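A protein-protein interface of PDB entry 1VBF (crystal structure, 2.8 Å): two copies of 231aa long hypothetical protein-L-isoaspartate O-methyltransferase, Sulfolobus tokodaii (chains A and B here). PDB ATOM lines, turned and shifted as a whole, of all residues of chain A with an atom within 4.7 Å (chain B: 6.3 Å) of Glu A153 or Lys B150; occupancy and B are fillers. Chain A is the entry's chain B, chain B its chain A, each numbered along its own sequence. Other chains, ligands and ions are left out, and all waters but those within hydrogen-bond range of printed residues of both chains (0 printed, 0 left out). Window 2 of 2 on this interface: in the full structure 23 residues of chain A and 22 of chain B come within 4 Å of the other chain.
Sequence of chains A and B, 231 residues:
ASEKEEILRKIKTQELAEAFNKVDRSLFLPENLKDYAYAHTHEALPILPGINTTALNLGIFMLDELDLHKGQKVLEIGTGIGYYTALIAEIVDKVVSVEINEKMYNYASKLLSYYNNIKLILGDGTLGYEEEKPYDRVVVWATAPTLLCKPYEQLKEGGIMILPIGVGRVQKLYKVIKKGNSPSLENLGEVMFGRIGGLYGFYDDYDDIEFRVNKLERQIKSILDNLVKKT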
ATOM      1  N   LYS A 133       3.571 -17.853  24.731  1.00  0.00           N
ATOM      2  CA  LYS A 133       4.600 -17.901  23.721  1.00  0.00           C
ATOM      3  C   LYS A 133       5.380 -16.723  23.266  1.00  0.00           C
ATOM      4  O   LYS A 133       6.538 -16.612  23.639  1.00  0.00           O
ATOM      5  CB  LYS A 133       4.120 -18.613  22.452  1.00  0.00           C
ATOM      6  CG  LYS A 133       5.289 -19.226  21.689  1.00  0.00           C
ATOM      7  CD  LYS A 133       4.844 -19.969  20.440  1.00  0.00           C
ATOM      8  CE  LYS A 133       4.735 -19.007  19.261  1.00  0.00           C
ATOM      9  NZ  LYS A 133       6.025 -18.281  18.971  1.00  0.00           N
ATOM     10  N   CYS A 149      17.302 -23.550  24.012  1.00  0.00           N
ATOM     11  CA  CYS A 149      16.469 -23.686  22.842  1.00  0.00           C
ATOM     12  C   CYS A 149      14.992 -23.282  22.961  1.00  0.00           C
ATOM     13  O   CYS A 149      14.492 -22.545  22.120  1.00  0.00           O
ATOM     14  CB  CYS A 149      16.627 -25.127  22.421  1.00  0.00           C
ATOM     15  SG  CYS A 149      15.591 -25.897  21.145  1.00  0.00           S
ATOM     16  N   LYS A 150      14.285 -23.753  23.979  1.00  0.00           N
ATOM     17  CA  LYS A 150      12.876 -23.386  24.117  1.00  0.00           C
ATOM     18  C   LYS A 150      12.696 -21.870  24.290  1.00  0.00           C
ATOM     19  O   LYS A 150      11.926 -21.240  23.560  1.00  0.00           O
ATOM     20  CB  LYS A 150      12.227 -24.125  25.296  1.00  0.00           C
ATOM     21  CG  LYS A 150      12.169 -25.605  25.118  1.00  0.00           C
ATOM     22  CD  LYS A 150      11.486 -25.968  23.819  1.00  0.00           C
ATOM     23  CE  LYS A 150      11.363 -27.473  23.688  1.00  0.00           C
ATOM     24  NZ  LYS A 150      10.582 -27.903  22.499  1.00  0.00           N
ATOM     25  N   PRO A 151      13.394 -21.264  25.269  1.00  0.00           N
ATOM     26  CA  PRO A 151      13.254 -19.813  25.455  1.00  0.00           C
ATOM     27  C   PRO A 151      13.534 -19.101  24.129  1.00  0.00           C
ATOM     28  O   PRO A 151      12.739 -18.291  23.663  1.00  0.00           O
ATOM     29  CB  PRO A 151      14.313 -19.498  26.499  1.00  0.00           C
ATOM     30  CG  PRO A 151      14.366 -20.765  27.308  1.00  0.00           C
ATOM     31  CD  PRO A 151      14.321 -21.840  26.254  1.00  0.00           C
ATOM     32  N   TYR A 152      14.667 -19.429  23.516  1.00  0.00           N
ATOM     33  CA  TYR A 152      15.019 -18.832  22.245  1.00  0.00           C
ATOM     34  C   TYR A 152      13.900 -18.981  21.206  1.00  0.00           C
ATOM     35  O   TYR A 152      13.634 -18.043  20.445  1.00  0.00           O
ATOM     36  CB  TYR A 152      16.304 -19.450  21.688  1.00  0.00           C
ATOM     37  CG  TYR A 152      16.790 -18.759  20.430  1.00  0.00           C
ATOM     38  CD1 TYR A 152      17.518 -17.578  20.500  1.00  0.00           C
ATOM     39  CD2 TYR A 152      16.448 -19.246  19.172  1.00  0.00           C
ATOM     40  CE1 TYR A 152      17.886 -16.892  19.341  1.00  0.00           C
ATOM     41  CE2 TYR A 152      16.808 -18.577  18.014  1.00  0.00           C
ATOM     42  CZ  TYR A 152      17.522 -17.398  18.092  1.00  0.00           C
ATOM     43  OH  TYR A 152      17.843 -16.723  16.924  1.00  0.00           O
ATOM     44  N   GLU A 153      13.250 -20.144  21.153  1.00  0.00           N
ATOM     45  CA  GLU A 153      12.182 -20.327  20.168  1.00  0.00           C
ATOM     46  C   GLU A 153      11.001 -19.441  20.537  1.00  0.00           C
ATOM     47  O   GLU A 153      10.346 -18.864  19.672  1.00  0.00           O
ATOM     48  CB  GLU A 153      11.696 -21.781  20.110  1.00  0.00           C
ATOM     49  CG  GLU A 153      12.780 -22.818  19.901  1.00  0.00           C
ATOM     50  CD  GLU A 153      12.240 -24.247  19.928  1.00  0.00           C
ATOM     51  OE1 GLU A 153      11.455 -24.595  20.851  1.00  0.00           O
ATOM     52  OE2 GLU A 153      12.624 -25.024  19.020  1.00  0.00           O
ATOM     53  N   GLN A 154      10.733 -19.341  21.831  1.00  0.00           N
ATOM     54  CA  GLN A 154       9.636 -18.533  22.319  1.00  0.00           C
ATOM     55  C   GLN A 154       9.861 -17.002  22.163  1.00  0.00           C
ATOM     56  O   GLN A 154       8.924 -16.211  22.235  1.00  0.00           O
ATOM     57  CB  GLN A 154       9.365 -18.939  23.769  1.00  0.00           C
ATOM     58  CG  GLN A 154       8.723 -20.321  23.882  1.00  0.00           C
ATOM     59  CD  GLN A 154       8.916 -20.972  25.240  1.00  0.00           C
ATOM     60  OE1 GLN A 154       8.879 -20.316  26.274  1.00  0.00           O
ATOM     61  NE2 GLN A 154       9.108 -22.279  25.238  1.00  0.00           N
ATOM     62  N   LEU A 155      11.096 -16.586  21.924  1.00  0.00           N
ATOM     63  CA  LEU A 155      11.405 -15.168  21.727  1.00  0.00           C
ATOM     64  C   LEU A 155      10.769 -14.621  20.453  1.00  0.00           C
ATOM     65  O   LEU A 155      10.582 -15.349  19.486  1.00  0.00           O
ATOM     66  CB  LEU A 155      12.913 -14.961  21.594  1.00  0.00           C
ATOM     67  CG  LEU A 155      13.650 -14.285  22.733  1.00  0.00           C
ATOM     68  CD1 LEU A 155      15.043 -13.915  22.269  1.00  0.00           C
ATOM     69  CD2 LEU A 155      12.896 -13.052  23.151  1.00  0.00           C
ATOM     70  N   LYS A 178      17.532 -12.314  18.712  1.00  0.00           N
ATOM     71  CA  LYS A 178      17.012 -13.258  17.753  1.00  0.00           C
ATOM     72  C   LYS A 178      17.034 -12.801  16.300  1.00  0.00           C
ATOM     73  O   LYS A 178      16.747 -11.641  15.984  1.00  0.00           O
ATOM     74  CB  LYS A 178      15.605 -13.679  18.145  1.00  0.00           C
ATOM     75  CG  LYS A 178      15.110 -14.875  17.374  1.00  0.00           C
ATOM     76  CD  LYS A 178      13.867 -15.399  18.021  1.00  0.00           C
ATOM     77  CE  LYS A 178      13.299 -16.612  17.313  1.00  0.00           C
ATOM     78  NZ  LYS A 178      12.049 -17.042  18.019  1.00  0.00           N
ATOM     79  N   LEU B  75      17.793 -38.842  10.097  1.00  0.00           N
ATOM     80  CA  LEU B  75      18.548 -37.601  10.199  1.00  0.00           C
ATOM     81  C   LEU B  75      19.936 -37.930  10.765  1.00  0.00           C
ATOM     82  O   LEU B  75      20.060 -38.410  11.887  1.00  0.00           O
ATOM     83  CB  LEU B  75      17.823 -36.611  11.114  1.00  0.00           C
ATOM     84  CG  LEU B  75      18.538 -35.265  11.259  1.00  0.00           C
ATOM     85  CD1 LEU B  75      18.593 -34.551   9.930  1.00  0.00           C
ATOM     86  CD2 LEU B  75      17.824 -34.421  12.289  1.00  0.00           C
ATOM     87  N   GLY B 125      24.421 -28.847  12.017  1.00  0.00           N
ATOM     88  CA  GLY B 125      23.673 -30.047  12.371  1.00  0.00           C
ATOM     89  C   GLY B 125      23.048 -29.936  13.744  1.00  0.00           C
ATOM     90  O   GLY B 125      22.199 -30.725  14.153  1.00  0.00           O
ATOM     91  N   THR B 126      23.476 -28.922  14.463  1.00  0.00           N
ATOM     92  CA  THR B 126      22.964 -28.703  15.795  1.00  0.00           C
ATOM     93  C   THR B 126      21.522 -28.180  15.750  1.00  0.00           C
ATOM     94  O   THR B 126      20.806 -28.200  16.747  1.00  0.00           O
ATOM     95  CB  THR B 126      23.924 -27.758  16.534  1.00  0.00           C
ATOM     96  OG1 THR B 126      24.344 -28.398  17.742  1.00  0.00           O
ATOM     97  CG2 THR B 126      23.293 -26.417  16.815  1.00  0.00           C
ATOM     98  N   LEU B 127      21.111 -27.737  14.568  1.00  0.00           N
ATOM     99  CA  LEU B 127      19.775 -27.218  14.333  1.00  0.00           C
ATOM    100  C   LEU B 127      18.936 -28.340  13.736  1.00  0.00           C
ATOM    101  O   LEU B 127      17.733 -28.191  13.536  1.00  0.00           O
ATOM    102  CB  LEU B 127      19.819 -26.100  13.302  1.00  0.00           C
ATOM    103  CG  LEU B 127      20.710 -24.889  13.509  1.00  0.00           C
ATOM    104  CD1 LEU B 127      20.860 -24.170  12.190  1.00  0.00           C
ATOM    105  CD2 LEU B 127      20.116 -24.008  14.587  1.00  0.00           C
ATOM    106  N   GLY B 128      19.592 -29.457  13.432  1.00  0.00           N
ATOM    107  CA  GLY B 128      18.909 -30.577  12.813  1.00  0.00           C
ATOM    108  C   GLY B 128      18.522 -30.144  11.417  1.00  0.00           C
ATOM    109  O   GLY B 128      19.325 -29.546  10.712  1.00  0.00           O
ATOM    110  N   TYR B 129      17.294 -30.443  11.010  1.00  0.00           N
ATOM    111  CA  TYR B 129      16.825 -30.025   9.698  1.00  0.00           C
ATOM    112  C   TYR B 129      15.317 -29.934   9.671  1.00  0.00           C
ATOM    113  O   TYR B 129      14.634 -30.883   9.314  1.00  0.00           O
ATOM    114  CB  TYR B 129      17.291 -30.983   8.622  1.00  0.00           C
ATOM    115  CG  TYR B 129      17.214 -30.342   7.271  1.00  0.00           C
ATOM    116  CD1 TYR B 129      18.011 -29.239   6.970  1.00  0.00           C
ATOM    117  CD2 TYR B 129      16.345 -30.821   6.290  1.00  0.00           C
ATOM    118  CE1 TYR B 129      17.951 -28.626   5.734  1.00  0.00           C
ATOM    119  CE2 TYR B 129      16.283 -30.218   5.042  1.00  0.00           C
ATOM    120  CZ  TYR B 129      17.094 -29.117   4.771  1.00  0.00           C
ATOM    121  OH  TYR B 129      17.062 -28.512   3.537  1.00  0.00           O
ATOM    122  N   LYS B 133      11.214 -32.103   8.744  1.00  0.00           N
ATOM    123  CA  LYS B 133      10.897 -32.332  10.122  1.00  0.00           C
ATOM    124  C   LYS B 133      10.605 -33.735  10.644  1.00  0.00           C
ATOM    125  O   LYS B 133      11.404 -34.206  11.453  1.00  0.00           O
ATOM    126  CB  LYS B 133       9.749 -31.381  10.624  1.00  0.00           C
ATOM    127  CG  LYS B 133       9.569 -31.347  12.153  1.00  0.00           C
ATOM    128  CD  LYS B 133       9.518 -29.911  12.742  1.00  0.00           C
ATOM    129  CE  LYS B 133       9.983 -29.887  14.202  1.00  0.00           C
ATOM    130  NZ  LYS B 133      10.080 -28.542  14.811  1.00  0.00           N
ATOM    131  N   LEU B 147      20.983 -32.818  25.790  1.00  0.00           N
ATOM    132  CA  LEU B 147      20.147 -33.500  24.827  1.00  0.00           C
ATOM    133  C   LEU B 147      20.015 -32.458  23.720  1.00  0.00           C
ATOM    134  O   LEU B 147      19.689 -31.315  24.012  1.00  0.00           O
ATOM    135  CB  LEU B 147      18.767 -33.721  25.427  1.00  0.00           C
ATOM    136  CG  LEU B 147      17.997 -35.005  25.165  1.00  0.00           C
ATOM    137  CD1 LEU B 147      16.527 -34.649  25.343  1.00  0.00           C
ATOM    138  CD2 LEU B 147      18.280 -35.587  23.770  1.00  0.00           C
ATOM    139  N   LEU B 148      20.278 -32.827  22.472  1.00  0.00           N
ATOM    140  CA  LEU B 148      20.153 -31.889  21.361  1.00  0.00           C
ATOM    141  C   LEU B 148      18.678 -31.629  21.066  1.00  0.00           C
ATOM    142  O   LEU B 148      17.985 -32.466  20.496  1.00  0.00           O
ATOM    143  CB  LEU B 148      20.826 -32.444  20.113  1.00  0.00           C
ATOM    144  CG  LEU B 148      22.348 -32.388  20.022  1.00  0.00           C
ATOM    145  CD1 LEU B 148      22.793 -33.056  18.739  1.00  0.00           C
ATOM    146  CD2 LEU B 148      22.810 -30.946  20.048  1.00  0.00           C
ATOM    147  N   CYS B 149      18.223 -30.447  21.449  1.00  0.00           N
ATOM    148  CA  CYS B 149      16.845 -29.996  21.299  1.00  0.00           C
ATOM    149  C   CYS B 149      16.241 -30.055  19.894  1.00  0.00           C
ATOM    150  O   CYS B 149      15.213 -30.684  19.692  1.00  0.00           O
ATOM    151  CB  CYS B 149      16.783 -28.575  21.843  1.00  0.00           C
ATOM    152  SG  CYS B 149      15.194 -27.699  22.048  1.00  0.00           S
ATOM    153  N   LYS B 150      16.863 -29.400  18.924  1.00  0.00           N
ATOM    154  CA  LYS B 150      16.321 -29.408  17.581  1.00  0.00           C
ATOM    155  C   LYS B 150      16.107 -30.800  17.008  1.00  0.00           C
ATOM    156  O   LYS B 150      15.011 -31.130  16.555  1.00  0.00           O
ATOM    157  CB  LYS B 150      17.201 -28.588  16.656  1.00  0.00           C
ATOM    158  CG  LYS B 150      17.159 -27.124  16.988  1.00  0.00           C
ATOM    159  CD  LYS B 150      15.731 -26.637  17.020  1.00  0.00           C
ATOM    160  CE  LYS B 150      15.656 -25.127  16.980  1.00  0.00           C
ATOM    161  NZ  LYS B 150      14.242 -24.636  17.051  1.00  0.00           N
ATOM    162  N   PRO B 151      17.157 -31.635  16.992  1.00  0.00           N
ATOM    163  CA  PRO B 151      16.954 -32.983  16.448  1.00  0.00           C
ATOM    164  C   PRO B 151      15.885 -33.741  17.242  1.00  0.00           C
ATOM    165  O   PRO B 151      15.066 -34.429  16.664  1.00  0.00           O
ATOM    166  CB  PRO B 151      18.339 -33.607  16.563  1.00  0.00           C
ATOM    167  CG  PRO B 151      19.251 -32.413  16.362  1.00  0.00           C
ATOM    168  CD  PRO B 151      18.591 -31.373  17.230  1.00  0.00           C
ATOM    169  N   TYR B 152      15.888 -33.605  18.563  1.00  0.00           N
ATOM    170  CA  TYR B 152      14.887 -34.268  19.406  1.00  0.00           C
ATOM    171  C   TYR B 152      13.465 -33.791  19.079  1.00  0.00           C
ATOM    172  O   TYR B 152      12.521 -34.578  19.070  1.00  0.00           O
ATOM    173  CB  TYR B 152      15.167 -33.993  20.881  1.00  0.00           C
ATOM    174  CG  TYR B 152      14.182 -34.649  21.812  1.00  0.00           C
ATOM    175  CD1 TYR B 152      14.219 -36.023  22.036  1.00  0.00           C
ATOM    176  CD2 TYR B 152      13.198 -33.902  22.460  1.00  0.00           C
ATOM    177  CE1 TYR B 152      13.308 -36.645  22.878  1.00  0.00           C
ATOM    178  CE2 TYR B 152      12.280 -34.511  23.305  1.00  0.00           C
ATOM    179  CZ  TYR B 152      12.342 -35.888  23.509  1.00  0.00           C
ATOM    180  OH  TYR B 152      11.441 -36.522  24.342  1.00  0.00           O
ATOM    181  N   GLU B 153      13.308 -32.494  18.839  1.00  0.00           N
ATOM    182  CA  GLU B 153      12.002 -31.956  18.497  1.00  0.00           C
ATOM    183  C   GLU B 153      11.548 -32.561  17.176  1.00  0.00           C
ATOM    184  O   GLU B 153      10.389 -32.908  17.007  1.00  0.00           O
ATOM    185  CB  GLU B 153      12.059 -30.443  18.328  1.00  0.00           C
ATOM    186  CG  GLU B 153      12.432 -29.669  19.569  1.00  0.00           C
ATOM    187  CD  GLU B 153      12.421 -28.155  19.343  1.00  0.00           C
ATOM    188  OE1 GLU B 153      12.803 -27.684  18.238  1.00  0.00           O
ATOM    189  OE2 GLU B 153      12.037 -27.438  20.292  1.00  0.00           O
ATOM    190  N   GLN B 154      12.471 -32.673  16.235  1.00  0.00           N
ATOM    191  CA  GLN B 154      12.167 -33.215  14.925  1.00  0.00           C
ATOM    192  C   GLN B 154      11.990 -34.753  14.874  1.00  0.00           C
ATOM    193  O   GLN B 154      11.908 -35.355  13.801  1.00  0.00           O
ATOM    194  CB  GLN B 154      13.264 -32.754  13.964  1.00  0.00           C
ATOM    195  CG  GLN B 154      13.262 -31.268  13.798  1.00  0.00           C
ATOM    196  CD  GLN B 154      14.551 -30.728  13.249  1.00  0.00           C
ATOM    197  OE1 GLN B 154      15.162 -31.317  12.353  1.00  0.00           O
ATOM    198  NE2 GLN B 154      14.968 -29.580  13.766  1.00  0.00           N
ATOM    199  N   LEU B 155      11.917 -35.389  16.029  1.00  0.00           N
ATOM    200  CA  LEU B 155      11.744 -36.830  16.056  1.00  0.00           C
ATOM    201  C   LEU B 155      10.269 -37.197  16.064  1.00  0.00           C
ATOM    202  O   LEU B 155       9.441 -36.403  16.484  1.00  0.00           O
ATOM    203  CB  LEU B 155      12.378 -37.408  17.320  1.00  0.00           C
ATOM    204  CG  LEU B 155      13.706 -38.149  17.267  1.00  0.00           C
ATOM    205  CD1 LEU B 155      13.955 -38.749  18.630  1.00  0.00           C
ATOM    206  CD2 LEU B 155      13.663 -39.251  16.238  1.00  0.00           C
ATOM    207  N   TYR B 200      23.716 -24.747  19.054  1.00  0.00           N
ATOM    208  CA  TYR B 200      23.415 -25.489  20.275  1.00  0.00           C
ATOM    209  C   TYR B 200      24.523 -26.462  20.597  1.00  0.00           C
ATOM    210  O   TYR B 200      24.279 -27.565  21.089  1.00  0.00           O
ATOM    211  CB  TYR B 200      22.080 -26.224  20.133  1.00  0.00           C
ATOM    212  CG  TYR B 200      20.947 -25.264  19.848  1.00  0.00           C
ATOM    213  CD1 TYR B 200      20.464 -24.414  20.841  1.00  0.00           C
ATOM    214  CD2 TYR B 200      20.427 -25.130  18.563  1.00  0.00           C
ATOM    215  CE1 TYR B 200      19.490 -23.446  20.560  1.00  0.00           C
ATOM    216  CE2 TYR B 200      19.466 -24.172  18.266  1.00  0.00           C
ATOM    217  CZ  TYR B 200      18.994 -23.328  19.269  1.00  0.00           C
ATOM    218  OH  TYR B 200      18.011 -22.390  18.990  1.00  0.00           O
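SG of Cys B149 forms a disulfide with SG of Cys A149 (2.1 Å). The side-chain carboxylate of Glu A153 lies close to the side-chain carboxylate of Glu B153 (2.8 Å). The side-chain carboxylate of Glu B153 lies within salt-bridge range of the side-chain amino group of Lys A150 (2.7 Å). NZ of Lys B150 is in salt-bridge range of OE2 of Glu A153.
O of Lys A150 sits close to NE2 of Gln A154 (3.4 Å). O of Glu A153 lies within hydrogen-bond range of NZ of Lys A178. The backbone carbonyl oxygen (O) of Tyr A152 sits at hydrogen-bond distance from the side-chain amino group (NZ) of Lys A178 (3.1 Å). NZ of Lys B150 lies within salt-bridge range of OE1 of Glu B153 (3.6 Å). NE2 of Gln B154 is in hydrogen-bond range of O of Lys B150 (3.2 Å). The side-chain amino group (NZ) of Lys A150 lies within salt-bridge range of the side-chain carboxylate (OE1) of Glu A153, at 3.8 Å.
OE2 of Glu B153 touches SG of Cys A149 (3.97 Å). Cys A149 touches Tyr B200 (CA to CE1, 3.8 Å). Tyr A152 touches Tyr B200.
Printed residues of chain B within 4 Å of Cys A149: Cys B149 (2.1 Å), Glu B153 (3.97 Å) and Tyr B200 (3.8 Å). Of the printed residues of chain B, Lys A150 touches Glu B153 (2.7 Å). Printed residues of chain B within 4 Å of Tyr A152: Tyr B200. Glu A153 touches just these residues of chain B: Lys B150 and Glu B153. Printed residues of chain A within 4 Å of Tyr B200: Cys A149 and Tyr A152. The nearest residue of chain A that does not touch Lys B150 is Cys A149 (4.2 Å). The nearest printed residue of chain B that does not touch Lys A150 is Cys B149 (4.2 Å).
Of the 17 printed residues of chain B, 4 touch a printed residue of chain A. Hydrophobic or aromatic side chains of chain A within 4 Å of the printed part of chain B: Tyr A152. Among the printed residues, Asp or Glu carboxylates within 4 Å of a Lys or Arg side-chain nitrogen of the other chain: Lys A150 with Glu B153 (2.7 Å) and Glu A153 with Lys B150 (2.6 Å).
Cys A149 touches its own counterpart, Cys B149. Cys A149 touches Glu B153, but with the chains exchanged Glu A153 does not touch Cys B149 (4.8 Å). Lys A150 touches Glu B153, and with the chains exchanged Glu A153 touches Lys B150. Glu A153 touches its own counterpart, Glu B153.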
